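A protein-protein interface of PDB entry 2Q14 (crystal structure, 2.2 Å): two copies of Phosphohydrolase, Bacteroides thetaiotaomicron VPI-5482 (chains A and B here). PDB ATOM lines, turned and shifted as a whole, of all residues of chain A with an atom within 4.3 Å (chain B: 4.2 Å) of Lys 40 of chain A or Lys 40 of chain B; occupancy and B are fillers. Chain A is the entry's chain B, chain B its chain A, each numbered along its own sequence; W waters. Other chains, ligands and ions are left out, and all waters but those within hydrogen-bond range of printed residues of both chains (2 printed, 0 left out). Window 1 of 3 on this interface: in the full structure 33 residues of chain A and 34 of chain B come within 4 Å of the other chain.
Of the 10 printed residues of chain B, 3 touch a printed residue of chain A.
Printed residues of chain B that touch a printed residue of chain A: Lys 40, Gln 53 and Thr 55.
Among the printed residues, 6 pairs touch across the chains.
Among the printed residues, no Asp or Glu carboxylate lies within 4 Å of a Lys or Arg side-chain nitrogen of the other chain.
The backbone carbonyl oxygen (O) of Gln 53 of chain B is in hydrogen-bond range of the side-chain amino group (NZ) of Lys 40 of chain B, at 2.6 Å.
The side-chain carboxylate (OD2) of Asp 286 of chain A is in hydrogen-bond range of the backbone NH (N) of Lys 40 of chain A.
N of Lys 40 of chain B is in hydrogen-bond range of OD2 of Asp 286 of chain B.
The side-chain amino group (NZ) of Lys 40 of chain A lies within hydrogen-bond range of the backbone carbonyl oxygen (O) of Gln 53 of chain A, 2.7 Å away.
Among the printed residues, pairs that only touch across the chains: Gln 53 of chain A with Gln 53 of chain B, Gln 53 of chain A with Thr 55 of chain B and Thr 55 of chain A with Gln 53 of chain B.
Water W2 bridges OG1 of Thr 55 of chain B and NE2 of Gln 53 of chain A.
Water W1 bridges OG1 of Thr 55 of chain A (2.7 Å) and NE2 of Gln 53 of chain B (3.2 Å).
Lys 40 of chain A touches its own counterpart, Lys 40 of chain B.
Lys 40 of chain A touches Gln 53 of chain B, and with the chains exchanged Gln 53 of chain A touches Lys 40 of chain B.
Gln 53 of chain A touches its own counterpart, Gln 53 of chain B.
Gln 53 of chain A touches Thr 55 of chain B, and with the chains exchanged Thr 55 of chain A touches Gln 53 of chain B.
Of chain B, only Lys 40 (2.9 Å) and Gln 53 (3.1 Å) come within 4 Å of Lys 40 of chain A.
Printed residues of chain B within 4 Å of Gln 53 of chain A: Lys 40, Gln 53 and Thr 55.
Of the printed residues of chain B, Thr 55 of chain A touches Gln 53.
Of chain A, only Lys 40 and Gln 53 come within 4 Å of Lys 40 of chain B.
Gln 41 of chain B touches none of the printed residues of chain A.
Of the printed residues of chain A, Gln 53 of chain B touches Lys 40, Gln 53 and Thr 55.
His 54 of chain B touches none of the printed residues of chain A.
Printed residues of chain A within 4 Å of Thr 55 of chain B: Gln 53 (3.6 Å).
The nearest printed residue of chain B that does not touch Lys 40 of chain A is His 54 of chain B (6.4 Å).
The nearest printed residue of chain A that does not touch Lys 40 of chain B is His 54 of chain A (6.5 Å).
The side-chain amino group (NZ) of Lys 40 of chain B lies within hydrogen-bond range of the side-chain amide oxygen (OE1) of Gln 53 of chain A (3.1 Å).
NZ of Lys 40 of chain A sits at hydrogen-bond distance from OE1 of Gln 53 of chain B (3.1 Å).
The side-chain amino group (NZ) of Lys 40 of chain A sits close to the side-chain amino group (NZ) of Lys 40 of chain B, 2.9 Å away.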
ATOM      1  N   ILE A  39      30.011 -19.955 -24.760  1.00  0.00           N
ATOM      2  CA  ILE A  39      29.285 -19.056 -23.872  1.00  0.00           C
ATOM      3  C   ILE A  39      27.793 -19.356 -24.002  1.00  0.00           C
ATOM      4  O   ILE A  39      27.234 -19.244 -25.092  1.00  0.00           O
ATOM      5  CB  ILE A  39      29.535 -17.556 -24.197  1.00  0.00           C
ATOM      6  CG1 ILE A  39      31.043 -17.237 -24.180  1.00  0.00           C
ATOM      7  CG2 ILE A  39      28.743 -16.668 -23.215  1.00  0.00           C
ATOM      8  CD1 ILE A  39      31.397 -15.846 -24.745  1.00  0.00           C
ATOM      9  N   LYS A  40      27.154 -19.700 -22.885  1.00  0.00           N
ATOM     10  CA  LYS A  40      25.723 -19.991 -22.853  1.00  0.00           C
ATOM     11  C   LYS A  40      24.921 -18.734 -22.978  1.00  0.00           C
ATOM     12  O   LYS A  40      25.290 -17.701 -22.464  1.00  0.00           O
ATOM     13  CB  LYS A  40      25.324 -20.729 -21.565  1.00  0.00           C
ATOM     14  CG  LYS A  40      26.018 -22.041 -21.288  1.00  0.00           C
ATOM     15  CD  LYS A  40      25.665 -23.090 -22.328  1.00  0.00           C
ATOM     16  CE  LYS A  40      26.517 -24.390 -22.213  1.00  0.00           C
ATOM     17  NZ  LYS A  40      26.466 -25.347 -23.407  1.00  0.00           N
ATOM     18  N   GLN A  41      23.810 -18.832 -23.683  1.00  0.00           N
ATOM     19  CA  GLN A  41      22.876 -17.735 -23.844  1.00  0.00           C
ATOM     20  C   GLN A  41      22.274 -17.334 -22.533  1.00  0.00           C
ATOM     21  O   GLN A  41      22.230 -16.144 -22.238  1.00  0.00           O
ATOM     22  CB  GLN A  41      21.774 -18.147 -24.796  1.00  0.00           C
ATOM     23  CG  GLN A  41      20.725 -17.106 -25.071  1.00  0.00           C
ATOM     24  CD  GLN A  41      21.185 -15.955 -25.937  1.00  0.00           C
ATOM     25  OE1 GLN A  41      22.149 -16.049 -26.697  1.00  0.00           O
ATOM     26  NE2 GLN A  41      20.466 -14.855 -25.837  1.00  0.00           N
ATOM     27  N   VAL A  42      21.806 -18.310 -21.750  1.00  0.00           N
ATOM     28  CA  VAL A  42      21.274 -18.046 -20.413  1.00  0.00           C
ATOM     29  C   VAL A  42      21.942 -18.944 -19.358  1.00  0.00           C
ATOM     30  O   VAL A  42      21.316 -19.837 -18.779  1.00  0.00           O
ATOM     31  CB  VAL A  42      19.730 -18.198 -20.366  1.00  0.00           C
ATOM     32  CG1 VAL A  42      19.101 -17.117 -21.138  1.00  0.00           C
ATOM     33  CG2 VAL A  42      19.283 -19.549 -20.908  1.00  0.00           C
ATOM     34  N   GLY A  43      23.219 -18.695 -19.099  1.00  0.00           N
ATOM     35  CA  GLY A  43      23.994 -19.556 -18.217  1.00  0.00           C
ATOM     36  C   GLY A  43      23.558 -19.644 -16.753  1.00  0.00           C
ATOM     37  O   GLY A  43      23.849 -20.618 -16.092  1.00  0.00           O
ATOM     38  N   GLN A  53      20.921 -25.275 -22.171  1.00  0.00           N
ATOM     39  CA  GLN A  53      22.335 -25.437 -22.451  1.00  0.00           C
ATOM     40  C   GLN A  53      22.727 -24.770 -23.760  1.00  0.00           C
ATOM     41  O   GLN A  53      23.871 -24.864 -24.173  1.00  0.00           O
ATOM     42  CB  GLN A  53      22.674 -26.940 -22.536  1.00  0.00           C
ATOM     43  CG  GLN A  53      22.389 -27.716 -21.232  1.00  0.00           C
ATOM     44  CD  GLN A  53      23.296 -27.265 -20.088  1.00  0.00           C
ATOM     45  OE1 GLN A  53      24.432 -26.900 -20.330  1.00  0.00           O
ATOM     46  NE2 GLN A  53      22.796 -27.284 -18.849  1.00  0.00           N
ATOM     47  N   HIS A  54      21.774 -24.096 -24.393  1.00  0.00           N
ATOM     48  CA  HIS A  54      22.010 -23.452 -25.669  1.00  0.00           C
ATOM     49  C   HIS A  54      23.019 -22.299 -25.591  1.00  0.00           C
ATOM     50  O   HIS A  54      23.131 -21.591 -24.568  1.00  0.00           O
ATOM     51  CB  HIS A  54      20.703 -23.023 -26.328  1.00  0.00           C
ATOM     52  CG  HIS A  54      19.879 -22.082 -25.507  1.00  0.00           C
ATOM     53  ND1 HIS A  54      19.378 -22.417 -24.270  1.00  0.00           N
ATOM     54  CD2 HIS A  54      19.467 -20.812 -25.748  1.00  0.00           C
ATOM     55  CE1 HIS A  54      18.693 -21.398 -23.784  1.00  0.00           C
ATOM     56  NE2 HIS A  54      18.715 -20.416 -24.667  1.00  0.00           N
ATOM     57  N   THR A  55      23.791 -22.161 -26.661  1.00  0.00           N
ATOM     58  CA  THR A  55      24.880 -21.190 -26.711  1.00  0.00           C
ATOM     59  C   THR A  55      24.527 -19.899 -27.456  1.00  0.00           C
ATOM     60  O   THR A  55      23.566 -19.835 -28.174  1.00  0.00           O
ATOM     61  CB  THR A  55      26.120 -21.819 -27.362  1.00  0.00           C
ATOM     62  OG1 THR A  55      25.932 -21.937 -28.783  1.00  0.00           O
ATOM     63  CG2 THR A  55      26.396 -23.207 -26.732  1.00  0.00           C
ATOM     64  N   ARG A  56      25.334 -18.872 -27.265  1.00  0.00           N
ATOM     65  CA  ARG A  56      25.182 -17.637 -27.983  1.00  0.00           C
ATOM     66  C   ARG A  56      25.428 -17.835 -29.488  1.00  0.00           C
ATOM     67  O   ARG A  56      24.807 -17.177 -30.309  1.00  0.00           O
ATOM     68  CB  ARG A  56      26.091 -16.577 -27.393  1.00  0.00           C
ATOM     69  CG  ARG A  56      25.725 -16.227 -25.920  1.00  0.00           C
ATOM     70  CD  ARG A  56      26.293 -14.874 -25.566  1.00  0.00           C
ATOM     71  NE  ARG A  56      25.958 -14.445 -24.224  1.00  0.00           N
ATOM     72  CZ  ARG A  56      24.815 -13.854 -23.868  1.00  0.00           C
ATOM     73  NH1 ARG A  56      23.856 -13.613 -24.738  1.00  0.00           N
ATOM     74  NH2 ARG A  56      24.631 -13.507 -22.615  1.00  0.00           N
ATOM     75  N   ASP A 286      32.945 -19.353 -20.784  1.00  0.00           N
ATOM     76  CA  ASP A 286      32.376 -19.994 -19.597  1.00  0.00           C
ATOM     77  C   ASP A 286      33.372 -20.891 -18.902  1.00  0.00           C
ATOM     78  O   ASP A 286      33.363 -20.995 -17.696  1.00  0.00           O
ATOM     79  CB  ASP A 286      31.132 -20.781 -19.962  1.00  0.00           C
ATOM     80  CG  ASP A 286      29.927 -19.876 -20.279  1.00  0.00           C
ATOM     81  OD1 ASP A 286      30.040 -18.642 -20.306  1.00  0.00           O
ATOM     82  OD2 ASP A 286      28.840 -20.402 -20.515  1.00  0.00           O
ATOM     83  N   ILE B  39      29.537 -32.071 -17.873  1.00  0.00           N
ATOM     84  CA  ILE B  39      30.013 -33.030 -18.855  1.00  0.00           C
ATOM     85  C   ILE B  39      28.920 -33.266 -19.905  1.00  0.00           C
ATOM     86  O   ILE B  39      27.825 -33.747 -19.592  1.00  0.00           O
ATOM     87  CB  ILE B  39      30.381 -34.365 -18.185  1.00  0.00           C
ATOM     88  CG1 ILE B  39      31.430 -34.145 -17.102  1.00  0.00           C
ATOM     89  CG2 ILE B  39      30.834 -35.392 -19.218  1.00  0.00           C
ATOM     90  CD1 ILE B  39      31.778 -35.379 -16.297  1.00  0.00           C
ATOM     91  N   LYS B  40      29.229 -32.951 -21.151  1.00  0.00           N
ATOM     92  CA  LYS B  40      28.302 -33.151 -22.237  1.00  0.00           C
ATOM     93  C   LYS B  40      28.069 -34.637 -22.530  1.00  0.00           C
ATOM     94  O   LYS B  40      28.954 -35.444 -22.442  1.00  0.00           O
ATOM     95  CB  LYS B  40      28.779 -32.444 -23.513  1.00  0.00           C
ATOM     96  CG  LYS B  40      28.924 -30.927 -23.381  1.00  0.00           C
ATOM     97  CD  LYS B  40      27.611 -30.235 -23.001  1.00  0.00           C
ATOM     98  CE  LYS B  40      27.717 -28.678 -22.924  1.00  0.00           C
ATOM     99  NZ  LYS B  40      26.505 -28.011 -22.298  1.00  0.00           N
ATOM    100  N   GLN B  41      26.843 -34.950 -22.915  1.00  0.00           N
ATOM    101  CA  GLN B  41      26.475 -36.280 -23.342  1.00  0.00           C
ATOM    102  C   GLN B  41      27.201 -36.697 -24.633  1.00  0.00           C
ATOM    103  O   GLN B  41      27.709 -37.822 -24.717  1.00  0.00           O
ATOM    104  CB  GLN B  41      24.961 -36.349 -23.532  1.00  0.00           C
ATOM    105  CG  GLN B  41      24.451 -37.710 -23.940  1.00  0.00           C
ATOM    106  CD  GLN B  41      24.523 -38.781 -22.865  1.00  0.00           C
ATOM    107  OE1 GLN B  41      24.678 -38.501 -21.682  1.00  0.00           O
ATOM    108  NE2 GLN B  41      24.403 -40.032 -23.290  1.00  0.00           N
ATOM    109  N   VAL B  42      27.240 -35.801 -25.622  1.00  0.00           N
ATOM    110  CA  VAL B  42      27.957 -36.054 -26.897  1.00  0.00           C
ATOM    111  C   VAL B  42      28.862 -34.878 -27.291  1.00  0.00           C
ATOM    112  O   VAL B  42      28.617 -34.203 -28.277  1.00  0.00           O
ATOM    113  CB  VAL B  42      26.983 -36.352 -28.066  1.00  0.00           C
ATOM    114  CG1 VAL B  42      26.463 -37.759 -27.980  1.00  0.00           C
ATOM    115  CG2 VAL B  42      25.871 -35.363 -28.076  1.00  0.00           C
ATOM    116  N   GLY B  43      29.894 -34.640 -26.496  1.00  0.00           N
ATOM    117  CA  GLY B  43      30.744 -33.447 -26.636  1.00  0.00           C
ATOM    118  C   GLY B  43      31.456 -33.292 -27.965  1.00  0.00           C
ATOM    119  O   GLY B  43      31.773 -32.178 -28.386  1.00  0.00           O
ATOM    120  N   GLN B  53      24.170 -29.708 -27.033  1.00  0.00           N
ATOM    121  CA  GLN B  53      24.718 -29.104 -25.817  1.00  0.00           C
ATOM    122  C   GLN B  53      24.259 -29.805 -24.531  1.00  0.00           C
ATOM    123  O   GLN B  53      24.650 -29.435 -23.461  1.00  0.00           O
ATOM    124  CB  GLN B  53      24.294 -27.631 -25.776  1.00  0.00           C
ATOM    125  CG  GLN B  53      24.776 -26.832 -26.980  1.00  0.00           C
ATOM    126  CD  GLN B  53      26.282 -26.804 -27.054  1.00  0.00           C
ATOM    127  OE1 GLN B  53      26.950 -26.863 -26.024  1.00  0.00           O
ATOM    128  NE2 GLN B  53      26.826 -26.745 -28.261  1.00  0.00           N
ATOM    129  N   HIS B  54      23.431 -30.830 -24.666  1.00  0.00           N
ATOM    130  CA  HIS B  54      22.889 -31.545 -23.524  1.00  0.00           C
ATOM    131  C   HIS B  54      23.939 -32.273 -22.723  1.00  0.00           C
ATOM    132  O   HIS B  54      24.908 -32.763 -23.249  1.00  0.00           O
ATOM    133  CB  HIS B  54      21.744 -32.495 -23.912  1.00  0.00           C
ATOM    134  CG  HIS B  54      22.096 -33.450 -24.999  1.00  0.00           C
ATOM    135  ND1 HIS B  54      22.354 -33.046 -26.296  1.00  0.00           N
ATOM    136  CD2 HIS B  54      22.201 -34.794 -24.997  1.00  0.00           C
ATOM    137  CE1 HIS B  54      22.642 -34.104 -27.033  1.00  0.00           C
ATOM    138  NE2 HIS B  54      22.570 -35.174 -26.265  1.00  0.00           N
ATOM    139  N   THR B  55      23.673 -32.363 -21.421  1.00  0.00           N
ATOM    140  CA  THR B  55      24.623 -32.863 -20.449  1.00  0.00           C
ATOM    141  C   THR B  55      24.291 -34.286 -20.030  1.00  0.00           C
ATOM    142  O   THR B  55      23.159 -34.769 -20.227  1.00  0.00           O
ATOM    143  CB  THR B  55      24.647 -31.958 -19.221  1.00  0.00           C
ATOM    144  OG1 THR B  55      23.434 -32.112 -18.486  1.00  0.00           O
ATOM    145  CG2 THR B  55      24.831 -30.480 -19.648  1.00  0.00           C
ATOM    146  N   ARG B  56      25.287 -34.972 -19.489  1.00  0.00           N
ATOM    147  CA  ARG B  56      25.050 -36.279 -18.881  1.00  0.00           C
ATOM    148  C   ARG B  56      24.071 -36.257 -17.713  1.00  0.00           C
ATOM    149  O   ARG B  56      23.462 -37.273 -17.419  1.00  0.00           O
ATOM    150  CB  ARG B  56      26.350 -36.905 -18.414  1.00  0.00           C
ATOM    151  CG  ARG B  56      27.240 -37.247 -19.533  1.00  0.00           C
ATOM    152  CD  ARG B  56      28.381 -38.115 -19.067  1.00  0.00           C
ATOM    153  NE  ARG B  56      29.282 -38.370 -20.176  1.00  0.00           N
ATOM    154  CZ  ARG B  56      29.038 -39.199 -21.185  1.00  0.00           C
ATOM    155  NH1 ARG B  56      27.915 -39.905 -21.247  1.00  0.00           N
ATOM    156  NH2 ARG B  56      29.927 -39.333 -22.142  1.00  0.00           N
ATOM    157  N   ASP B 286      34.314 -31.081 -18.324  1.00  0.00           N
ATOM    158  CA  ASP B 286      34.679 -30.527 -19.626  1.00  0.00           C
ATOM    159  C   ASP B 286      35.467 -29.223 -19.491  1.00  0.00           C
ATOM    160  O   ASP B 286      36.272 -28.926 -20.342  1.00  0.00           O
ATOM    161  CB  ASP B 286      33.447 -30.263 -20.513  1.00  0.00           C
ATOM    162  CG  ASP B 286      32.690 -31.520 -20.902  1.00  0.00           C
ATOM    163  OD1 ASP B 286      33.180 -32.664 -20.692  1.00  0.00           O
ATOM    164  OD2 ASP B 286      31.566 -31.339 -21.419  1.00  0.00           O
HETATM  165  O   HOH W   1      26.540 -24.169 -30.214  1.00  0.00           O
HETATM  166  O   HOH W   2      22.076 -30.113 -17.314  1.00  0.00           O
